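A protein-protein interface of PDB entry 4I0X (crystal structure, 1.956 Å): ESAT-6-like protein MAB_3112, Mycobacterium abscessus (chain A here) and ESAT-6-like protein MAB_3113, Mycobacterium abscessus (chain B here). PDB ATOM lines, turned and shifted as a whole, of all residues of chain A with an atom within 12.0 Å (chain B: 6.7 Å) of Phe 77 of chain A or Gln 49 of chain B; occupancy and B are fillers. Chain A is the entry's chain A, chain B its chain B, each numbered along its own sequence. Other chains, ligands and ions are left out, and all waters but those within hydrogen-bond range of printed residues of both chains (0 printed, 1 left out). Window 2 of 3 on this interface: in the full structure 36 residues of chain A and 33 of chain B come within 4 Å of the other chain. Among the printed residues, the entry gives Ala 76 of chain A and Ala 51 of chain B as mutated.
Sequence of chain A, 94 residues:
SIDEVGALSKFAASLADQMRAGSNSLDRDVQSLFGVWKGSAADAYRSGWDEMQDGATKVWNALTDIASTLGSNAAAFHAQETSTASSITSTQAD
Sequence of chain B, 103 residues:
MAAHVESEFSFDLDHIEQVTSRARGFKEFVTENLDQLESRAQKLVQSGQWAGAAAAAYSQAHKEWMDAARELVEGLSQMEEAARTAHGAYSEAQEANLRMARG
The indole nitrogen (NE1) of Trp 50 of chain B lies within hydrogen-bond range of the backbone carbonyl oxygen (O) of Phe 77 of chain A, 3.3 Å away.
NE2 of Gln 49 of chain B lies within hydrogen-bond range of O of Phe 77 of chain A, at 3.3 Å.
Among the printed residues, pairs that only touch across the chains: Ala 76 of chain A with Ala 54 of chain B, Phe 77 of chain A with Ala 54 of chain B, Leu 70 of chain A with Trp 50 of chain B, Val 5 of chain A with Gln 49 of chain B, Val 5 of chain A with Trp 50 of chain B and Glu 4 of chain A with Leu 44 of chain B.
The backbone carbonyl oxygen (O) of Leu 44 of chain B sits at hydrogen-bond distance from the backbone NH (N) of Trp 50 of chain B.
The backbone carbonyl oxygen of Leu 44 of chain B is in hydrogen-bond range of the backbone NH of Gln 49 of chain B (3.1 Å).
The backbone carbonyl oxygen (O) of Leu 44 of chain B lies within hydrogen-bond range of the side-chain hydroxyl (OG) of Ser 47 of chain B (3.0 Å).
N of Gln 49 of chain B sits close to OG of Ser 47 of chain B (3.3 Å).
Printed residues of chain B within 4 Å of Glu 4 of chain A: Leu 44 (3.95 Å).
Printed residues of chain B within 4 Å of Val 5 of chain A: Gln 49 and Trp 50.
Gly 6 of chain A touches none of the printed residues of chain B.
Ala 12 of chain A touches none of the printed residues of chain B.
Of chain A, only Glu 4 comes within 4 Å of Leu 44 of chain B.
No residue of chain A comes within 4 Å of Gly 48 of chain B.
Gln 49 of chain B touches two residues of chain A.
Printed residues of chain A within 4 Å of Trp 50 of chain B: Val 5 (3.8 Å), Leu 70 (3.7 Å) and Phe 77 (3.3 Å).
Ala 51 of chain B touches none of the printed residues of chain A.
No residue of chain A comes within 4 Å of Ala 53 of chain B.
Ala 54 of chain B touches just these residues of chain A: Ala 76 (3.3 Å) and Phe 77 (3.3 Å).
No residue of chain A comes within 4 Å of Ala 57 of chain B.
The nearest residue of chain B that does not touch Phe 77 of chain A is Ala 57 of chain B (4.03 Å).
The nearest residue of chain A that does not touch Gln 49 of chain B is Ala 76 of chain A (5.0 Å).
The nearest printed residue of chain B that does not touch Val 5 of chain A is Leu 44 of chain B (4.6 Å).
Of the 14 printed residues of chain B, 4 touch a printed residue of chain A.
Hydrophobic or aromatic side chains of chain B that line the printed part of chain A: Leu 44, Trp 50 and Ala 54.
Of the 25 printed residues of chain A, 5 touch a printed residue of chain B.
Printed residues of chain A that touch a printed residue of chain B: Glu 4, Val 5, Leu 70, Ala 76 and Phe 77.
Among the printed residues, no Asp or Glu carboxylate lies within 4 Å of a Lys or Arg side-chain nitrogen of the other chain.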
ATOM      1  N   ASP A   3     -24.353 -28.720 -22.320  1.00  0.00           N
ATOM      2  CA  ASP A   3     -23.479 -29.643 -21.604  1.00  0.00           C
ATOM      3  C   ASP A   3     -22.087 -29.551 -22.181  1.00  0.00           C
ATOM      4  O   ASP A   3     -21.111 -29.741 -21.468  1.00  0.00           O
ATOM      5  CB  ASP A   3     -23.985 -31.083 -21.709  1.00  0.00           C
ATOM      6  CG  ASP A   3     -23.025 -32.096 -21.083  1.00  0.00           C
ATOM      7  OD1 ASP A   3     -22.965 -32.187 -19.835  1.00  0.00           O
ATOM      8  OD2 ASP A   3     -22.339 -32.817 -21.843  1.00  0.00           O
ATOM      9  N   GLU A   4     -21.992 -29.263 -23.475  1.00  0.00           N
ATOM     10  CA  GLU A   4     -20.689 -29.050 -24.091  1.00  0.00           C
ATOM     11  C   GLU A   4     -19.972 -27.876 -23.419  1.00  0.00           C
ATOM     12  O   GLU A   4     -18.746 -27.861 -23.334  1.00  0.00           O
ATOM     13  CB  GLU A   4     -20.827 -28.823 -25.592  1.00  0.00           C
ATOM     14  CG  GLU A   4     -19.524 -28.599 -26.322  1.00  0.00           C
ATOM     15  CD  GLU A   4     -18.655 -29.861 -26.437  1.00  0.00           C
ATOM     16  OE1 GLU A   4     -18.029 -30.066 -27.505  1.00  0.00           O
ATOM     17  OE2 GLU A   4     -18.583 -30.635 -25.460  1.00  0.00           O
ATOM     18  N   VAL A   5     -20.725 -26.916 -22.890  1.00  0.00           N
ATOM     19  CA  VAL A   5     -20.091 -25.772 -22.224  1.00  0.00           C
ATOM     20  C   VAL A   5     -19.385 -26.203 -20.951  1.00  0.00           C
ATOM     21  O   VAL A   5     -18.209 -25.891 -20.757  1.00  0.00           O
ATOM     22  CB  VAL A   5     -21.115 -24.682 -21.890  1.00  0.00           C
ATOM     23  CG1 VAL A   5     -20.469 -23.595 -21.064  1.00  0.00           C
ATOM     24  CG2 VAL A   5     -21.691 -24.107 -23.179  1.00  0.00           C
ATOM     25  N   GLY A   6     -20.106 -26.916 -20.085  1.00  0.00           N
ATOM     26  CA  GLY A   6     -19.515 -27.566 -18.926  1.00  0.00           C
ATOM     27  C   GLY A   6     -18.361 -28.497 -19.285  1.00  0.00           C
ATOM     28  O   GLY A   6     -17.337 -28.552 -18.576  1.00  0.00           O
ATOM     29  N   ALA A   7     -18.480 -29.222 -20.391  1.00  0.00           N
ATOM     30  CA  ALA A   7     -17.404 -30.138 -20.784  1.00  0.00           C
ATOM     31  C   ALA A   7     -16.122 -29.391 -21.171  1.00  0.00           C
ATOM     32  O   ALA A   7     -14.988 -29.809 -20.838  1.00  0.00           O
ATOM     33  CB  ALA A   7     -17.857 -31.068 -21.910  1.00  0.00           C
ATOM     34  N   LEU A   8     -16.279 -28.276 -21.863  1.00  0.00           N
ATOM     35  CA  LEU A   8     -15.107 -27.509 -22.262  1.00  0.00           C
ATOM     36  C   LEU A   8     -14.475 -26.806 -21.083  1.00  0.00           C
ATOM     37  O   LEU A   8     -13.271 -26.625 -21.056  1.00  0.00           O
ATOM     38  CB  LEU A   8     -15.469 -26.488 -23.345  1.00  0.00           C
ATOM     39  CG  LEU A   8     -15.818 -27.158 -24.673  1.00  0.00           C
ATOM     40  CD1 LEU A   8     -16.257 -26.139 -25.709  1.00  0.00           C
ATOM     41  CD2 LEU A   8     -14.639 -27.947 -25.176  1.00  0.00           C
ATOM     42  N   SER A   9     -15.284 -26.384 -20.117  1.00  0.00           N
ATOM     43  CA  SER A   9     -14.723 -25.779 -18.929  1.00  0.00           C
ATOM     44  C   SER A   9     -13.853 -26.773 -18.175  1.00  0.00           C
ATOM     45  O   SER A   9     -12.792 -26.419 -17.660  1.00  0.00           O
ATOM     46  CB  SER A   9     -15.807 -25.233 -18.017  1.00  0.00           C
ATOM     47  OG  SER A   9     -15.213 -24.670 -16.858  1.00  0.00           O
ATOM     48  N   LYS A  10     -14.312 -28.010 -18.095  1.00  0.00           N
ATOM     49  CA  LYS A  10     -13.583 -29.064 -17.390  1.00  0.00           C
ATOM     50  C   LYS A  10     -12.354 -29.434 -18.174  1.00  0.00           C
ATOM     51  O   LYS A  10     -11.277 -29.680 -17.605  1.00  0.00           O
ATOM     52  CB  LYS A  10     -14.455 -30.299 -17.162  1.00  0.00           C
ATOM     53  CG  LYS A  10     -15.613 -30.041 -16.227  1.00  0.00           C
ATOM     54  CD  LYS A  10     -16.440 -31.297 -15.980  1.00  0.00           C
ATOM     55  CE  LYS A  10     -15.727 -32.194 -14.991  1.00  0.00           C
ATOM     56  NZ  LYS A  10     -16.545 -33.360 -14.592  1.00  0.00           N
ATOM     57  N   ALA A  12     -10.595 -27.468 -20.356  1.00  0.00           N
ATOM     58  CA  ALA A  12      -9.615 -26.393 -20.220  1.00  0.00           C
ATOM     59  C   ALA A  12      -8.941 -26.402 -18.821  1.00  0.00           C
ATOM     60  O   ALA A  12      -7.740 -26.215 -18.698  1.00  0.00           O
ATOM     61  CB  ALA A  12     -10.297 -25.061 -20.472  1.00  0.00           C
ATOM     62  N   ALA A  62      -4.336 -18.503 -19.951  1.00  0.00           N
ATOM     63  CA  ALA A  62      -5.466 -18.340 -20.863  1.00  0.00           C
ATOM     64  C   ALA A  62      -6.474 -19.461 -20.654  1.00  0.00           C
ATOM     65  O   ALA A  62      -7.678 -19.209 -20.653  1.00  0.00           O
ATOM     66  CB  ALA A  62      -5.000 -18.300 -22.309  1.00  0.00           C
ATOM     67  N   LEU A  63      -5.983 -20.673 -20.447  1.00  0.00           N
ATOM     68  CA  LEU A  63      -6.840 -21.831 -20.164  1.00  0.00           C
ATOM     69  C   LEU A  63      -7.641 -21.682 -18.879  1.00  0.00           C
ATOM     70  O   LEU A  63      -8.805 -21.955 -18.850  1.00  0.00           O
ATOM     71  CB  LEU A  63      -6.030 -23.146 -20.085  1.00  0.00           C
ATOM     72  CG  LEU A  63      -5.523 -23.633 -21.427  1.00  0.00           C
ATOM     73  CD1 LEU A  63      -4.502 -24.709 -21.254  1.00  0.00           C
ATOM     74  CD2 LEU A  63      -6.670 -24.119 -22.329  1.00  0.00           C
ATOM     75  N   THR A  64      -6.994 -21.246 -17.830  1.00  0.00           N
ATOM     76  CA  THR A  64      -7.627 -21.002 -16.565  1.00  0.00           C
ATOM     77  C   THR A  64      -8.690 -19.930 -16.655  1.00  0.00           C
ATOM     78  O   THR A  64      -9.750 -20.062 -16.069  1.00  0.00           O
ATOM     79  CB  THR A  64      -6.548 -20.569 -15.546  1.00  0.00           C
ATOM     80  OG1 THR A  64      -5.666 -21.684 -15.313  1.00  0.00           O
ATOM     81  CG2 THR A  64      -7.154 -20.146 -14.283  1.00  0.00           C
ATOM     82  N   ASP A  65      -8.384 -18.850 -17.358  1.00  0.00           N
ATOM     83  CA  ASP A  65      -9.358 -17.785 -17.575  1.00  0.00           C
ATOM     84  C   ASP A  65     -10.588 -18.301 -18.290  1.00  0.00           C
ATOM     85  O   ASP A  65     -11.677 -18.099 -17.826  1.00  0.00           O
ATOM     86  CB  ASP A  65      -8.757 -16.630 -18.381  1.00  0.00           C
ATOM     87  CG  ASP A  65      -7.643 -15.922 -17.645  1.00  0.00           C
ATOM     88  OD1 ASP A  65      -7.539 -16.085 -16.406  1.00  0.00           O
ATOM     89  OD2 ASP A  65      -6.868 -15.199 -18.311  1.00  0.00           O
ATOM     90  N   ILE A  66     -10.435 -18.956 -19.430  1.00  0.00           N
ATOM     91  CA  ILE A  66     -11.634 -19.363 -20.150  1.00  0.00           C
ATOM     92  C   ILE A  66     -12.360 -20.441 -19.348  1.00  0.00           C
ATOM     93  O   ILE A  66     -13.570 -20.506 -19.367  1.00  0.00           O
ATOM     94  CB  ILE A  66     -11.314 -19.859 -21.601  1.00  0.00           C
ATOM     95  CG1 ILE A  66     -12.559 -19.918 -22.488  1.00  0.00           C
ATOM     96  CG2 ILE A  66     -10.691 -21.227 -21.575  1.00  0.00           C
ATOM     97  CD1 ILE A  66     -13.414 -18.721 -22.440  1.00  0.00           C
ATOM     98  N   ALA A  67     -11.622 -21.305 -18.669  1.00  0.00           N
ATOM     99  CA  ALA A  67     -12.269 -22.351 -17.857  1.00  0.00           C
ATOM    100  C   ALA A  67     -13.176 -21.710 -16.824  1.00  0.00           C
ATOM    101  O   ALA A  67     -14.305 -22.122 -16.651  1.00  0.00           O
ATOM    102  CB  ALA A  67     -11.231 -23.250 -17.188  1.00  0.00           C
ATOM    103  N   SER A  68     -12.675 -20.699 -16.133  1.00  0.00           N
ATOM    104  CA  SER A  68     -13.439 -20.017 -15.081  1.00  0.00           C
ATOM    105  C   SER A  68     -14.650 -19.279 -15.629  1.00  0.00           C
ATOM    106  O   SER A  68     -15.733 -19.346 -15.058  1.00  0.00           O
ATOM    107  CB  SER A  68     -12.530 -19.042 -14.359  1.00  0.00           C
ATOM    108  OG  SER A  68     -11.457 -19.765 -13.790  1.00  0.00           O
ATOM    109  N   THR A  69     -14.449 -18.546 -16.720  1.00  0.00           N
ATOM    110  CA  THR A  69     -15.541 -17.806 -17.345  1.00  0.00           C
ATOM    111  C   THR A  69     -16.635 -18.759 -17.793  1.00  0.00           C
ATOM    112  O   THR A  69     -17.808 -18.517 -17.546  1.00  0.00           O
ATOM    113  CB  THR A  69     -15.019 -16.936 -18.504  1.00  0.00           C
ATOM    114  OG1 THR A  69     -14.021 -16.058 -17.993  1.00  0.00           O
ATOM    115  CG2 THR A  69     -16.111 -16.093 -19.099  1.00  0.00           C
ATOM    116  N   LEU A  70     -16.271 -19.855 -18.437  1.00  0.00           N
ATOM    117  CA  LEU A  70     -17.272 -20.845 -18.844  1.00  0.00           C
ATOM    118  C   LEU A  70     -17.943 -21.530 -17.650  1.00  0.00           C
ATOM    119  O   LEU A  70     -19.095 -21.901 -17.723  1.00  0.00           O
ATOM    120  CB  LEU A  70     -16.613 -21.925 -19.704  1.00  0.00           C
ATOM    121  CG  LEU A  70     -16.179 -21.561 -21.120  1.00  0.00           C
ATOM    122  CD1 LEU A  70     -15.490 -22.769 -21.689  1.00  0.00           C
ATOM    123  CD2 LEU A  70     -17.393 -21.157 -21.969  1.00  0.00           C
ATOM    124  N   GLY A  71     -17.201 -21.763 -16.574  1.00  0.00           N
ATOM    125  CA  GLY A  71     -17.777 -22.394 -15.406  1.00  0.00           C
ATOM    126  C   GLY A  71     -18.651 -21.443 -14.634  1.00  0.00           C
ATOM    127  O   GLY A  71     -19.760 -21.792 -14.230  1.00  0.00           O
ATOM    128  N   SER A  72     -18.189 -20.214 -14.454  1.00  0.00           N
ATOM    129  CA  SER A  72     -18.936 -19.279 -13.619  1.00  0.00           C
ATOM    130  C   SER A  72     -20.007 -18.506 -14.395  1.00  0.00           C
ATOM    131  O   SER A  72     -21.044 -18.163 -13.817  1.00  0.00           O
ATOM    132  CB  SER A  72     -17.992 -18.318 -12.888  1.00  0.00           C
ATOM    133  OG  SER A  72     -17.691 -17.200 -13.696  1.00  0.00           O
ATOM    134  N   ASN A  73     -19.789 -18.233 -15.682  1.00  0.00           N
ATOM    135  CA  ASN A  73     -20.818 -17.529 -16.492  1.00  0.00           C
ATOM    136  C   ASN A  73     -21.492 -18.422 -17.545  1.00  0.00           C
ATOM    137  O   ASN A  73     -21.808 -17.980 -18.659  1.00  0.00           O
ATOM    138  CB  ASN A  73     -20.234 -16.265 -17.142  1.00  0.00           C
ATOM    139  CG  ASN A  73     -19.534 -15.357 -16.124  1.00  0.00           C
ATOM    140  OD1 ASN A  73     -18.306 -15.373 -16.001  1.00  0.00           O
ATOM    141  ND2 ASN A  73     -20.317 -14.599 -15.367  1.00  0.00           N
ATOM    142  N   ALA A  74     -21.733 -19.675 -17.171  1.00  0.00           N
ATOM    143  CA  ALA A  74     -22.310 -20.654 -18.083  1.00  0.00           C
ATOM    144  C   ALA A  74     -23.494 -20.123 -18.906  1.00  0.00           C
ATOM    145  O   ALA A  74     -23.586 -20.417 -20.096  1.00  0.00           O
ATOM    146  CB  ALA A  74     -22.717 -21.910 -17.315  1.00  0.00           C
ATOM    147  N   ALA A  75     -24.384 -19.343 -18.286  1.00  0.00           N
ATOM    148  CA  ALA A  75     -25.610 -18.860 -18.951  1.00  0.00           C
ATOM    149  C   ALA A  75     -25.391 -18.025 -20.223  1.00  0.00           C
ATOM    150  O   ALA A  75     -26.206 -18.078 -21.151  1.00  0.00           O
ATOM    151  CB  ALA A  75     -26.441 -18.066 -17.983  1.00  0.00           C
ATOM    152  N   ALA A  76     -24.318 -17.234 -20.251  1.00  0.00           N
ATOM    153  CA  ALA A  76     -24.036 -16.344 -21.386  1.00  0.00           C
ATOM    154  C   ALA A  76     -23.472 -17.131 -22.572  1.00  0.00           C
ATOM    155  O   ALA A  76     -23.338 -16.602 -23.686  1.00  0.00           O
ATOM    156  CB  ALA A  76     -23.071 -15.227 -20.974  1.00  0.00           C
ATOM    157  N   PHE A  77     -23.136 -18.393 -22.322  1.00  0.00           N
ATOM    158  CA  PHE A  77     -22.622 -19.269 -23.360  1.00  0.00           C
ATOM    159  C   PHE A  77     -23.713 -20.223 -23.854  1.00  0.00           C
ATOM    160  O   PHE A  77     -23.424 -21.315 -24.332  1.00  0.00           O
ATOM    161  CB  PHE A  77     -21.406 -20.034 -22.831  1.00  0.00           C
ATOM    162  CG  PHE A  77     -20.198 -19.149 -22.582  1.00  0.00           C
ATOM    163  CD1 PHE A  77     -19.996 -18.550 -21.345  1.00  0.00           C
ATOM    164  CD2 PHE A  77     -19.281 -18.900 -23.592  1.00  0.00           C
ATOM    165  CE1 PHE A  77     -18.901 -17.728 -21.120  1.00  0.00           C
ATOM    166  CE2 PHE A  77     -18.172 -18.069 -23.376  1.00  0.00           C
ATOM    167  CZ  PHE A  77     -17.986 -17.488 -22.138  1.00  0.00           C
ATOM    168  N   LYS B  43     -16.787 -24.884 -33.155  1.00  0.00           N
ATOM    169  CA  LYS B  43     -18.128 -25.307 -33.567  1.00  0.00           C
ATOM    170  C   LYS B  43     -19.174 -24.425 -32.899  1.00  0.00           C
ATOM    171  O   LYS B  43     -20.162 -24.021 -33.549  1.00  0.00           O
ATOM    172  CB  LYS B  43     -18.392 -26.778 -33.263  1.00  0.00           C
ATOM    173  CG  LYS B  43     -17.544 -27.722 -34.109  1.00  0.00           C
ATOM    174  CD  LYS B  43     -17.866 -29.193 -33.859  1.00  0.00           C
ATOM    175  CE  LYS B  43     -16.896 -30.110 -34.606  1.00  0.00           C
ATOM    176  NZ  LYS B  43     -17.073 -30.065 -36.089  1.00  0.00           N
ATOM    177  N   LEU B  44     -18.982 -24.105 -31.621  1.00  0.00           N
ATOM    178  CA  LEU B  44     -20.014 -23.352 -30.899  1.00  0.00           C
ATOM    179  C   LEU B  44     -20.125 -21.913 -31.403  1.00  0.00           C
ATOM    180  O   LEU B  44     -21.205 -21.354 -31.456  1.00  0.00           O
ATOM    181  CB  LEU B  44     -19.753 -23.376 -29.389  1.00  0.00           C
ATOM    182  CG  LEU B  44     -19.724 -24.794 -28.800  1.00  0.00           C
ATOM    183  CD1 LEU B  44     -19.695 -24.767 -27.281  1.00  0.00           C
ATOM    184  CD2 LEU B  44     -20.916 -25.602 -29.306  1.00  0.00           C
ATOM    185  N   VAL B  45     -19.003 -21.304 -31.768  1.00  0.00           N
ATOM    186  CA  VAL B  45     -19.057 -19.967 -32.331  1.00  0.00           C
ATOM    187  C   VAL B  45     -19.693 -20.054 -33.709  1.00  0.00           C
ATOM    188  O   VAL B  45     -20.512 -19.213 -34.082  1.00  0.00           O
ATOM    189  CB  VAL B  45     -17.648 -19.307 -32.406  1.00  0.00           C
ATOM    190  CG1 VAL B  45     -17.743 -17.958 -33.036  1.00  0.00           C
ATOM    191  CG2 VAL B  45     -17.053 -19.153 -30.998  1.00  0.00           C
ATOM    192  N   GLN B  46     -19.326 -21.081 -34.461  1.00  0.00           N
ATOM    193  CA  GLN B  46     -19.859 -21.275 -35.803  1.00  0.00           C
ATOM    194  C   GLN B  46     -21.381 -21.420 -35.760  1.00  0.00           C
ATOM    195  O   GLN B  46     -22.098 -20.805 -36.566  1.00  0.00           O
ATOM    196  CB  GLN B  46     -19.229 -22.515 -36.435  1.00  0.00           C
ATOM    197  CG  GLN B  46     -19.859 -22.918 -37.762  1.00  0.00           C
ATOM    198  CD  GLN B  46     -19.536 -24.352 -38.180  1.00  0.00           C
ATOM    199  OE1 GLN B  46     -19.029 -25.153 -37.384  1.00  0.00           O
ATOM    200  NE2 GLN B  46     -19.843 -24.683 -39.438  1.00  0.00           N
ATOM    201  N   SER B  47     -21.886 -22.211 -34.812  1.00  0.00           N
ATOM    202  CA  SER B  47     -23.326 -22.463 -34.752  1.00  0.00           C
ATOM    203  C   SER B  47     -24.100 -21.227 -34.292  1.00  0.00           C
ATOM    204  O   SER B  47     -25.305 -21.169 -34.444  1.00  0.00           O
ATOM    205  CB  SER B  47     -23.629 -23.635 -33.817  1.00  0.00           C
ATOM    206  OG  SER B  47     -23.285 -23.324 -32.468  1.00  0.00           O
ATOM    207  N   GLY B  48     -23.405 -20.262 -33.695  1.00  0.00           N
ATOM    208  CA  GLY B  48     -24.047 -19.104 -33.106  1.00  0.00           C
ATOM    209  C   GLY B  48     -24.433 -19.258 -31.651  1.00  0.00           C
ATOM    210  O   GLY B  48     -24.967 -18.329 -31.045  1.00  0.00           O
ATOM    211  N   GLN B  49     -24.192 -20.429 -31.078  1.00  0.00           N
ATOM    212  CA  GLN B  49     -24.521 -20.645 -29.689  1.00  0.00           C
ATOM    213  C   GLN B  49     -23.655 -19.743 -28.843  1.00  0.00           C
ATOM    214  O   GLN B  49     -24.071 -19.343 -27.760  1.00  0.00           O
ATOM    215  CB  GLN B  49     -24.322 -22.101 -29.271  1.00  0.00           C
ATOM    216  CG  GLN B  49     -24.624 -22.338 -27.770  1.00  0.00           C
ATOM    217  CD  GLN B  49     -24.462 -23.792 -27.363  1.00  0.00           C
ATOM    218  OE1 GLN B  49     -24.784 -24.696 -28.137  1.00  0.00           O
ATOM    219  NE2 GLN B  49     -23.952 -24.025 -26.153  1.00  0.00           N
ATOM    220  N   TRP B  50     -22.442 -19.445 -29.322  1.00  0.00           N
ATOM    221  CA  TRP B  50     -21.575 -18.487 -28.646  1.00  0.00           C
ATOM    222  C   TRP B  50     -21.463 -17.259 -29.525  1.00  0.00           C
ATOM    223  O   TRP B  50     -20.789 -17.281 -30.559  1.00  0.00           O
ATOM    224  CB  TRP B  50     -20.162 -19.013 -28.413  1.00  0.00           C
ATOM    225  CG  TRP B  50     -20.020 -20.079 -27.386  1.00  0.00           C
ATOM    226  CD1 TRP B  50     -21.021 -20.698 -26.687  1.00  0.00           C
ATOM    227  CD2 TRP B  50     -18.801 -20.648 -26.935  1.00  0.00           C
ATOM    228  NE1 TRP B  50     -20.485 -21.627 -25.831  1.00  0.00           N
ATOM    229  CE2 TRP B  50     -19.122 -21.617 -25.969  1.00  0.00           C
ATOM    230  CE3 TRP B  50     -17.465 -20.442 -27.257  1.00  0.00           C
ATOM    231  CZ2 TRP B  50     -18.148 -22.378 -25.332  1.00  0.00           C
ATOM    232  CZ3 TRP B  50     -16.508 -21.197 -26.624  1.00  0.00           C
ATOM    233  CH2 TRP B  50     -16.848 -22.153 -25.678  1.00  0.00           C
ATOM    234  N   ALA B  51     -22.090 -16.189 -29.079  1.00  0.00           N
ATOM    235  CA  ALA B  51     -22.128 -14.924 -29.809  1.00  0.00           C
ATOM    236  C   ALA B  51     -21.866 -13.810 -28.805  1.00  0.00           C
ATOM    237  O   ALA B  51     -21.849 -14.056 -27.587  1.00  0.00           O
ATOM    238  CB  ALA B  51     -23.481 -14.735 -30.466  1.00  0.00           C
ATOM    239  N   ALA B  53     -20.610 -11.279 -26.173  1.00  0.00           N
ATOM    240  CA  ALA B  53     -19.611 -11.336 -25.096  1.00  0.00           C
ATOM    241  C   ALA B  53     -19.000 -12.719 -24.962  1.00  0.00           C
ATOM    242  O   ALA B  53     -17.784 -12.861 -24.694  1.00  0.00           O
ATOM    243  CB  ALA B  53     -20.231 -10.910 -23.783  1.00  0.00           C
ATOM    244  N   ALA B  54     -19.828 -13.738 -25.152  1.00  0.00           N
ATOM    245  CA  ALA B  54     -19.370 -15.138 -25.109  1.00  0.00           C
ATOM    246  C   ALA B  54     -18.288 -15.418 -26.134  1.00  0.00           C
ATOM    247  O   ALA B  54     -17.253 -16.017 -25.823  1.00  0.00           O
ATOM    248  CB  ALA B  54     -20.540 -16.099 -25.320  1.00  0.00           C
ATOM    249  N   ALA B  55     -18.526 -15.003 -27.369  1.00  0.00           N
ATOM    250  CA  ALA B  55     -17.497 -15.134 -28.401  1.00  0.00           C
ATOM    251  C   ALA B  55     -16.246 -14.295 -28.093  1.00  0.00           C
ATOM    252  O   ALA B  55     -15.127 -14.724 -28.353  1.00  0.00           O
ATOM    253  CB  ALA B  55     -18.072 -14.751 -29.778  1.00  0.00           C
ATOM    254  N   ALA B  57     -15.007 -13.590 -25.227  1.00  0.00           N
ATOM    255  CA  ALA B  57     -14.225 -14.247 -24.170  1.00  0.00           C
ATOM    256  C   ALA B  57     -13.393 -15.371 -24.769  1.00  0.00           C
ATOM    257  O   ALA B  57     -12.172 -15.487 -24.529  1.00  0.00           O
ATOM    258  CB  ALA B  57     -15.155 -14.778 -23.074  1.00  0.00           C
ATOM    259  N   TYR B  58     -14.033 -16.167 -25.614  1.00  0.00           N
ATOM    260  CA  TYR B  58     -13.320 -17.252 -26.259  1.00  0.00           C
ATOM    261  C   TYR B  58     -12.212 -16.707 -27.143  1.00  0.00           C
ATOM    262  O   TYR B  58     -11.072 -17.188 -27.129  1.00  0.00           O
ATOM    263  CB  TYR B  58     -14.236 -18.119 -27.117  1.00  0.00           C
ATOM    264  CG  TYR B  58     -13.408 -19.118 -27.866  1.00  0.00           C
ATOM    265  CD1 TYR B  58     -12.734 -20.124 -27.180  1.00  0.00           C
ATOM    266  CD2 TYR B  58     -13.244 -19.032 -29.242  1.00  0.00           C
ATOM    267  CE1 TYR B  58     -11.945 -21.022 -27.846  1.00  0.00           C
ATOM    268  CE2 TYR B  58     -12.453 -19.928 -29.918  1.00  0.00           C
ATOM    269  CZ  TYR B  58     -11.798 -20.921 -29.215  1.00  0.00           C
ATOM    270  OH  TYR B  58     -10.995 -21.829 -29.876  1.00  0.00           O
